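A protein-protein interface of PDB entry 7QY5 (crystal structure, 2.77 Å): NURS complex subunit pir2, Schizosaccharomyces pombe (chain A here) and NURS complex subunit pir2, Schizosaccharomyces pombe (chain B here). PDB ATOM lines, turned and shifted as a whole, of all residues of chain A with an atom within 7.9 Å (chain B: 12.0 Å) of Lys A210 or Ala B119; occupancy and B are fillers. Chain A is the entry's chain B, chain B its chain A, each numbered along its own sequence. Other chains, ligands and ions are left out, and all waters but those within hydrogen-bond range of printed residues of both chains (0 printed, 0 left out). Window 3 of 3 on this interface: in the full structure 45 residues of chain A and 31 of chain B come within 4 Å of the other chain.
Of the 18 printed residues of chain A, 5 touch a printed residue of chain B. Hydrophobic or aromatic side chains of chain A within 4 Å of the printed part of chain B: Ile A108. Along chain B the printed residues that touch a printed residue of chain A span positions 116 to 119. Among the printed residues, no Asp or Glu carboxylate lies within 4 Å of a Lys or Arg side-chain nitrogen of the other chain.
Among the printed residues, merely in contact across the chains: Ser A208 with Pro B117 (3.1 Å), Arg A209 with Thr B118 (3.3 Å), Tyr A207 with Leu B116 (3.5 Å), Tyr A207 with Pro B117 (3.5 Å), Lys A210 with Ala B119 (3.6 Å) and Ile A108 with Leu B116 (3.8 Å).
O of Ile A106 is in hydrogen-bond range of N of Ser A208, at 3.1 Å. The backbone carbonyl oxygen of Ser A208 is in hydrogen-bond range of the backbone NH of Ile A108, at 2.7 Å. The backbone NH (N) of Lys A210 sits at hydrogen-bond distance from the backbone carbonyl oxygen (O) of Ile A108. The guanidinium group of Arg A209 sits at hydrogen-bond distance from the backbone carbonyl oxygen of Ala A112, 3.3 Å away. The side-chain hydroxyl (OG) of Ser A113 is in hydrogen-bond range of the guanidinium group (NH1) of Arg A209 (3.3 Å). The side-chain hydroxyl (OG) of Ser A113 is in hydrogen-bond range of the backbone carbonyl oxygen (O) of Lys A210 (3.4 Å).
O of Pro B117 lies within hydrogen-bond range of N of Arg A209, at 2.8 Å. The backbone NH of Ala B119 lies within hydrogen-bond range of the backbone carbonyl oxygen of Arg A209 (3.1 Å).
Of chain B, only Leu B116 comes within 4 Å of Ile A108. No residue of chain B comes within 4 Å of Phe A109. No residue of chain B comes within 4 Å of Glu A110. Ile A111 touches none of the printed residues of chain B. No residue of chain B comes within 4 Å of Ala A112. Ser A113 touches none of the printed residues of chain B. Of the printed residues of chain B, Tyr A207 touches Leu B116 and Pro B117. Printed residues of chain B within 4 Å of Ser A208: Pro B117. Printed residues of chain B within 4 Å of Lys A210: Ala B119 (3.6 Å). No residue of chain B comes within 4 Å of Lys A211. Tyr B39 touches none of the printed residues of chain A. Printed residues of chain A within 4 Å of Leu B116: Ile A108 (3.8 Å) and Tyr A207 (3.5 Å). Of the printed residues of chain A, Ala B119 touches Arg A209 and Lys A210. The nearest residue of chain A that does not touch Ala B119 is Ser A208 (4.2 Å). The nearest printed residue of chain A that does not touch Leu B116 is Arg A209 (4.01 Å).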
ATOM      1  N   PRO A 105     -11.863  13.904   4.691  1.00  0.00           N
ATOM      2  CA  PRO A 105     -11.174  14.930   5.472  1.00  0.00           C
ATOM      3  C   PRO A 105     -12.066  15.550   6.558  1.00  0.00           C
ATOM      4  O   PRO A 105     -13.164  15.945   6.265  1.00  0.00           O
ATOM      5  CB  PRO A 105     -10.791  15.990   4.431  1.00  0.00           C
ATOM      6  CG  PRO A 105     -10.691  15.213   3.129  1.00  0.00           C
ATOM      7  CD  PRO A 105     -11.668  14.060   3.244  1.00  0.00           C
ATOM      8  N   ILE A 106     -11.556  15.628   7.783  1.00  0.00           N
ATOM      9  CA  ILE A 106     -12.281  16.183   8.961  1.00  0.00           C
ATOM     10  C   ILE A 106     -12.569  17.654   8.688  1.00  0.00           C
ATOM     11  O   ILE A 106     -11.651  18.465   8.629  1.00  0.00           O
ATOM     12  CB  ILE A 106     -11.440  16.000  10.234  1.00  0.00           C
ATOM     13  CG1 ILE A 106     -11.142  14.526  10.508  1.00  0.00           C
ATOM     14  CG2 ILE A 106     -12.099  16.662  11.421  1.00  0.00           C
ATOM     15  CD1 ILE A 106      -9.707  14.264  10.946  1.00  0.00           C
ATOM     16  N   PRO A 107     -13.844  18.059   8.531  1.00  0.00           N
ATOM     17  CA  PRO A 107     -14.160  19.452   8.204  1.00  0.00           C
ATOM     18  C   PRO A 107     -13.957  20.404   9.397  1.00  0.00           C
ATOM     19  O   PRO A 107     -14.441  20.113  10.458  1.00  0.00           O
ATOM     20  CB  PRO A 107     -15.628  19.378   7.758  1.00  0.00           C
ATOM     21  CG  PRO A 107     -16.187  18.184   8.521  1.00  0.00           C
ATOM     22  CD  PRO A 107     -15.036  17.214   8.695  1.00  0.00           C
ATOM     23  N   ILE A 108     -13.211  21.496   9.202  1.00  0.00           N
ATOM     24  CA  ILE A 108     -13.018  22.591  10.202  1.00  0.00           C
ATOM     25  C   ILE A 108     -14.185  23.576  10.071  1.00  0.00           C
ATOM     26  O   ILE A 108     -14.642  23.822   8.932  1.00  0.00           O
ATOM     27  CB  ILE A 108     -11.667  23.310  10.003  1.00  0.00           C
ATOM     28  CG1 ILE A 108     -10.486  22.346  10.135  1.00  0.00           C
ATOM     29  CG2 ILE A 108     -11.533  24.499  10.949  1.00  0.00           C
ATOM     30  CD1 ILE A 108      -9.226  22.828   9.462  1.00  0.00           C
ATOM     31  N   PHE A 109     -14.616  24.161  11.189  1.00  0.00           N
ATOM     32  CA  PHE A 109     -15.770  25.089  11.231  1.00  0.00           C
ATOM     33  C   PHE A 109     -15.491  26.302  10.352  1.00  0.00           C
ATOM     34  O   PHE A 109     -14.324  26.623  10.043  1.00  0.00           O
ATOM     35  CB  PHE A 109     -16.095  25.542  12.650  1.00  0.00           C
ATOM     36  CG  PHE A 109     -17.051  24.646  13.392  1.00  0.00           C
ATOM     37  CD1 PHE A 109     -18.200  24.172  12.780  1.00  0.00           C
ATOM     38  CD2 PHE A 109     -16.819  24.316  14.719  1.00  0.00           C
ATOM     39  CE1 PHE A 109     -19.078  23.358  13.477  1.00  0.00           C
ATOM     40  CE2 PHE A 109     -17.711  23.526  15.421  1.00  0.00           C
ATOM     41  CZ  PHE A 109     -18.833  23.039  14.796  1.00  0.00           C
ATOM     42  N   GLU A 110     -16.590  26.928   9.949  1.00  0.00           N
ATOM     43  CA  GLU A 110     -16.637  28.127   9.090  1.00  0.00           C
ATOM     44  C   GLU A 110     -15.743  29.211   9.713  1.00  0.00           C
ATOM     45  O   GLU A 110     -14.937  29.780   8.973  1.00  0.00           O
ATOM     46  CB  GLU A 110     -18.110  28.506   8.926  1.00  0.00           C
ATOM     47  CG  GLU A 110     -18.356  29.661   7.976  1.00  0.00           C
ATOM     48  CD  GLU A 110     -19.826  29.928   7.666  1.00  0.00           C
ATOM     49  OE1 GLU A 110     -20.225  31.125   7.561  1.00  0.00           O
ATOM     50  OE2 GLU A 110     -20.577  28.936   7.518  1.00  0.00           O
ATOM     51  N   ILE A 111     -15.820  29.421  11.036  1.00  0.00           N
ATOM     52  CA  ILE A 111     -15.208  30.576  11.782  1.00  0.00           C
ATOM     53  C   ILE A 111     -13.674  30.589  11.650  1.00  0.00           C
ATOM     54  O   ILE A 111     -13.088  31.676  11.793  1.00  0.00           O
ATOM     55  CB  ILE A 111     -15.644  30.599  13.268  1.00  0.00           C
ATOM     56  CG1 ILE A 111     -15.294  31.932  13.937  1.00  0.00           C
ATOM     57  CG2 ILE A 111     -15.064  29.419  14.037  1.00  0.00           C
ATOM     58  CD1 ILE A 111     -16.009  32.182  15.242  1.00  0.00           C
ATOM     59  N   ALA A 112     -13.040  29.439  11.393  1.00  0.00           N
ATOM     60  CA  ALA A 112     -11.571  29.309  11.233  1.00  0.00           C
ATOM     61  C   ALA A 112     -11.102  30.050   9.969  1.00  0.00           C
ATOM     62  O   ALA A 112      -9.885  30.387   9.852  1.00  0.00           O
ATOM     63  CB  ALA A 112     -11.212  27.849  11.185  1.00  0.00           C
ATOM     64  N   SER A 113     -12.041  30.288   9.055  1.00  0.00           N
ATOM     65  CA  SER A 113     -11.808  30.871   7.715  1.00  0.00           C
ATOM     66  C   SER A 113     -12.153  32.372   7.725  1.00  0.00           C
ATOM     67  O   SER A 113     -11.676  33.090   6.824  1.00  0.00           O
ATOM     68  CB  SER A 113     -12.597  30.076   6.701  1.00  0.00           C
ATOM     69  OG  SER A 113     -12.599  28.679   7.029  1.00  0.00           O
ATOM     70  N   SER A 114     -12.930  32.837   8.715  1.00  0.00           N
ATOM     71  CA  SER A 114     -13.279  34.269   8.955  1.00  0.00           C
ATOM     72  C   SER A 114     -12.015  35.055   9.271  1.00  0.00           C
ATOM     73  O   SER A 114     -11.113  34.486   9.882  1.00  0.00           O
ATOM     74  CB  SER A 114     -14.226  34.446  10.100  1.00  0.00           C
ATOM     75  OG  SER A 114     -13.498  34.699  11.303  1.00  0.00           O
ATOM     76  N   ILE A 169      -5.353  32.545   4.670  1.00  0.00           N
ATOM     77  CA  ILE A 169      -5.808  31.124   4.636  1.00  0.00           C
ATOM     78  C   ILE A 169      -4.680  30.255   4.068  1.00  0.00           C
ATOM     79  O   ILE A 169      -4.244  29.313   4.763  1.00  0.00           O
ATOM     80  CB  ILE A 169      -7.120  30.980   3.836  1.00  0.00           C
ATOM     81  CG1 ILE A 169      -8.321  31.481   4.640  1.00  0.00           C
ATOM     82  CG2 ILE A 169      -7.330  29.541   3.382  1.00  0.00           C
ATOM     83  CD1 ILE A 169      -9.589  31.577   3.838  1.00  0.00           C
ATOM     84  N   TYR A 207      -7.672  17.479   6.868  1.00  0.00           N
ATOM     85  CA  TYR A 207      -8.829  18.349   7.185  1.00  0.00           C
ATOM     86  C   TYR A 207      -9.311  19.070   5.931  1.00  0.00           C
ATOM     87  O   TYR A 207      -8.592  19.086   4.926  1.00  0.00           O
ATOM     88  CB  TYR A 207      -8.432  19.381   8.237  1.00  0.00           C
ATOM     89  CG  TYR A 207      -8.199  18.811   9.609  1.00  0.00           C
ATOM     90  CD1 TYR A 207      -9.174  18.908  10.590  1.00  0.00           C
ATOM     91  CD2 TYR A 207      -7.016  18.164   9.923  1.00  0.00           C
ATOM     92  CE1 TYR A 207      -8.975  18.388  11.856  1.00  0.00           C
ATOM     93  CE2 TYR A 207      -6.801  17.647  11.189  1.00  0.00           C
ATOM     94  CZ  TYR A 207      -7.780  17.766  12.159  1.00  0.00           C
ATOM     95  OH  TYR A 207      -7.576  17.259  13.407  1.00  0.00           O
ATOM     96  N   SER A 208     -10.502  19.660   6.021  1.00  0.00           N
ATOM     97  CA  SER A 208     -11.084  20.570   5.004  1.00  0.00           C
ATOM     98  C   SER A 208     -11.588  21.842   5.701  1.00  0.00           C
ATOM     99  O   SER A 208     -11.693  21.853   6.955  1.00  0.00           O
ATOM    100  CB  SER A 208     -12.170  19.884   4.215  1.00  0.00           C
ATOM    101  OG  SER A 208     -13.141  19.319   5.080  1.00  0.00           O
ATOM    102  N   ARG A 209     -11.845  22.890   4.911  1.00  0.00           N
ATOM    103  CA  ARG A 209     -12.384  24.186   5.394  1.00  0.00           C
ATOM    104  C   ARG A 209     -13.817  24.341   4.886  1.00  0.00           C
ATOM    105  O   ARG A 209     -14.014  24.218   3.671  1.00  0.00           O
ATOM    106  CB  ARG A 209     -11.493  25.339   4.926  1.00  0.00           C
ATOM    107  CG  ARG A 209     -10.254  25.553   5.784  1.00  0.00           C
ATOM    108  CD  ARG A 209      -9.275  26.514   5.140  1.00  0.00           C
ATOM    109  NE  ARG A 209      -8.153  26.864   6.001  1.00  0.00           N
ATOM    110  CZ  ARG A 209      -8.207  27.726   7.006  1.00  0.00           C
ATOM    111  NH1 ARG A 209      -9.343  28.343   7.300  1.00  0.00           N
ATOM    112  NH2 ARG A 209      -7.121  27.974   7.718  1.00  0.00           N
ATOM    113  N   LYS A 210     -14.771  24.586   5.790  1.00  0.00           N
ATOM    114  CA  LYS A 210     -16.151  24.999   5.427  1.00  0.00           C
ATOM    115  C   LYS A 210     -16.092  26.484   5.068  1.00  0.00           C
ATOM    116  O   LYS A 210     -15.438  27.222   5.826  1.00  0.00           O
ATOM    117  CB  LYS A 210     -17.128  24.691   6.565  1.00  0.00           C
ATOM    118  CG  LYS A 210     -17.606  23.244   6.617  1.00  0.00           C
ATOM    119  CD  LYS A 210     -18.194  22.823   7.954  1.00  0.00           C
ATOM    120  CE  LYS A 210     -19.632  23.252   8.150  1.00  0.00           C
ATOM    121  NZ  LYS A 210     -20.071  23.036   9.551  1.00  0.00           N
ATOM    122  N   LYS A 211     -16.684  26.874   3.931  1.00  0.00           N
ATOM    123  CA  LYS A 211     -16.522  28.218   3.306  1.00  0.00           C
ATOM    124  C   LYS A 211     -17.211  29.239   4.211  1.00  0.00           C
ATOM    125  O   LYS A 211     -18.232  28.877   4.823  1.00  0.00           O
ATOM    126  CB  LYS A 211     -17.100  28.236   1.883  1.00  0.00           C
ATOM    127  CG  LYS A 211     -16.982  29.557   1.128  1.00  0.00           C
ATOM    128  CD  LYS A 211     -15.651  29.766   0.436  1.00  0.00           C
ATOM    129  CE  LYS A 211     -15.476  31.175  -0.094  1.00  0.00           C
ATOM    130  NZ  LYS A 211     -14.255  31.291  -0.926  1.00  0.00           N
ATOM    131  N   PHE A 212     -16.658  30.447   4.315  1.00  0.00           N
ATOM    132  CA  PHE A 212     -17.229  31.553   5.122  1.00  0.00           C
ATOM    133  C   PHE A 212     -18.192  32.355   4.240  1.00  0.00           C
ATOM    134  O   PHE A 212     -17.733  32.918   3.225  1.00  0.00           O
ATOM    135  CB  PHE A 212     -16.116  32.420   5.715  1.00  0.00           C
ATOM    136  CG  PHE A 212     -16.611  33.492   6.650  1.00  0.00           C
ATOM    137  CD1 PHE A 212     -16.771  34.798   6.215  1.00  0.00           C
ATOM    138  CD2 PHE A 212     -16.950  33.187   7.959  1.00  0.00           C
ATOM    139  CE1 PHE A 212     -17.239  35.779   7.076  1.00  0.00           C
ATOM    140  CE2 PHE A 212     -17.422  34.168   8.818  1.00  0.00           C
ATOM    141  CZ  PHE A 212     -17.565  35.462   8.375  1.00  0.00           C
ATOM    142  N   ASN A 213     -19.485  32.355   4.585  1.00  0.00           N
ATOM    143  CA  ASN A 213     -20.499  33.268   3.993  1.00  0.00           C
ATOM    144  C   ASN A 213     -20.495  34.551   4.810  1.00  0.00           C
ATOM    145  O   ASN A 213     -20.839  34.542   5.990  1.00  0.00           O
ATOM    146  CB  ASN A 213     -21.894  32.650   3.943  1.00  0.00           C
ATOM    147  CG  ASN A 213     -22.039  31.607   2.858  1.00  0.00           C
ATOM    148  OD1 ASN A 213     -21.137  31.419   2.042  1.00  0.00           O
ATOM    149  ND2 ASN A 213     -23.172  30.926   2.838  1.00  0.00           N
ATOM    150  N   TYR B  39     -32.205  23.140  22.251  1.00  0.00           N
ATOM    151  CA  TYR B  39     -30.924  22.594  21.723  1.00  0.00           C
ATOM    152  C   TYR B  39     -29.898  23.722  21.518  1.00  0.00           C
ATOM    153  O   TYR B  39     -28.718  23.488  21.827  1.00  0.00           O
ATOM    154  CB  TYR B  39     -31.152  21.776  20.441  1.00  0.00           C
ATOM    155  CG  TYR B  39     -29.912  21.144  19.836  1.00  0.00           C
ATOM    156  CD1 TYR B  39     -29.044  21.879  19.031  1.00  0.00           C
ATOM    157  CD2 TYR B  39     -29.597  19.807  20.055  1.00  0.00           C
ATOM    158  CE1 TYR B  39     -27.905  21.317  18.472  1.00  0.00           C
ATOM    159  CE2 TYR B  39     -28.455  19.232  19.507  1.00  0.00           C
ATOM    160  CZ  TYR B  39     -27.604  19.990  18.715  1.00  0.00           C
ATOM    161  OH  TYR B  39     -26.475  19.451  18.166  1.00  0.00           O
ATOM    162  N   HIS B  43     -25.908  24.974  24.559  1.00  0.00           N
ATOM    163  CA  HIS B  43     -24.580  24.590  24.015  1.00  0.00           C
ATOM    164  C   HIS B  43     -23.488  24.994  25.019  1.00  0.00           C
ATOM    165  O   HIS B  43     -22.748  24.106  25.480  1.00  0.00           O
ATOM    166  CB  HIS B  43     -24.383  25.181  22.606  1.00  0.00           C
ATOM    167  CG  HIS B  43     -25.046  24.393  21.520  1.00  0.00           C
ATOM    168  ND1 HIS B  43     -25.131  23.007  21.555  1.00  0.00           N
ATOM    169  CD2 HIS B  43     -25.637  24.785  20.367  1.00  0.00           C
ATOM    170  CE1 HIS B  43     -25.749  22.585  20.476  1.00  0.00           C
ATOM    171  NE2 HIS B  43     -26.071  23.655  19.728  1.00  0.00           N
ATOM    172  N   GLN B 115      -3.148  23.766  -0.310  1.00  0.00           N
ATOM    173  CA  GLN B 115      -4.331  24.432   0.281  1.00  0.00           C
ATOM    174  C   GLN B 115      -5.293  23.368   0.844  1.00  0.00           C
ATOM    175  O   GLN B 115      -5.523  22.349   0.155  1.00  0.00           O
ATOM    176  CB  GLN B 115      -4.981  25.277  -0.815  1.00  0.00           C
ATOM    177  CG  GLN B 115      -6.411  25.683  -0.499  1.00  0.00           C
ATOM    178  CD  GLN B 115      -7.370  25.188  -1.550  1.00  0.00           C
ATOM    179  OE1 GLN B 115      -8.074  24.193  -1.359  1.00  0.00           O
ATOM    180  NE2 GLN B 115      -7.391  25.892  -2.669  1.00  0.00           N
ATOM    181  N   LEU B 116      -5.864  23.602   2.034  1.00  0.00           N
ATOM    182  CA  LEU B 116      -6.850  22.686   2.678  1.00  0.00           C
ATOM    183  C   LEU B 116      -8.101  22.616   1.809  1.00  0.00           C
ATOM    184  O   LEU B 116      -8.718  23.635   1.534  1.00  0.00           O
ATOM    185  CB  LEU B 116      -7.202  23.175   4.091  1.00  0.00           C
ATOM    186  CG  LEU B 116      -6.227  22.791   5.207  1.00  0.00           C
ATOM    187  CD1 LEU B 116      -6.789  23.135   6.577  1.00  0.00           C
ATOM    188  CD2 LEU B 116      -5.871  21.307   5.149  1.00  0.00           C
ATOM    189  N   PRO B 117      -8.531  21.425   1.345  1.00  0.00           N
ATOM    190  CA  PRO B 117      -9.718  21.338   0.496  1.00  0.00           C
ATOM    191  C   PRO B 117     -10.959  21.975   1.139  1.00  0.00           C
ATOM    192  O   PRO B 117     -10.962  22.180   2.355  1.00  0.00           O
ATOM    193  CB  PRO B 117      -9.942  19.835   0.295  1.00  0.00           C
ATOM    194  CG  PRO B 117      -9.064  19.165   1.337  1.00  0.00           C
ATOM    195  CD  PRO B 117      -7.923  20.117   1.616  1.00  0.00           C
ATOM    196  N   THR B 118     -11.970  22.279   0.316  1.00  0.00           N
ATOM    197  CA  THR B 118     -13.278  22.842   0.756  1.00  0.00           C
ATOM    198  C   THR B 118     -14.218  21.685   1.103  1.00  0.00           C
ATOM    199  O   THR B 118     -13.969  20.576   0.635  1.00  0.00           O
ATOM    200  CB  THR B 118     -13.846  23.794  -0.301  1.00  0.00           C
ATOM    201  OG1 THR B 118     -12.766  24.649  -0.673  1.00  0.00           O
ATOM    202  CG2 THR B 118     -15.008  24.632   0.190  1.00  0.00           C
ATOM    203  N   ALA B 119     -15.228  21.931   1.931  1.00  0.00           N
ATOM    204  CA  ALA B 119     -16.222  20.924   2.368  1.00  0.00           C
ATOM    205  C   ALA B 119     -17.415  20.928   1.399  1.00  0.00           C
ATOM    206  O   ALA B 119     -18.025  19.884   1.163  1.00  0.00           O
ATOM    207  CB  ALA B 119     -16.637  21.219   3.790  1.00  0.00           C
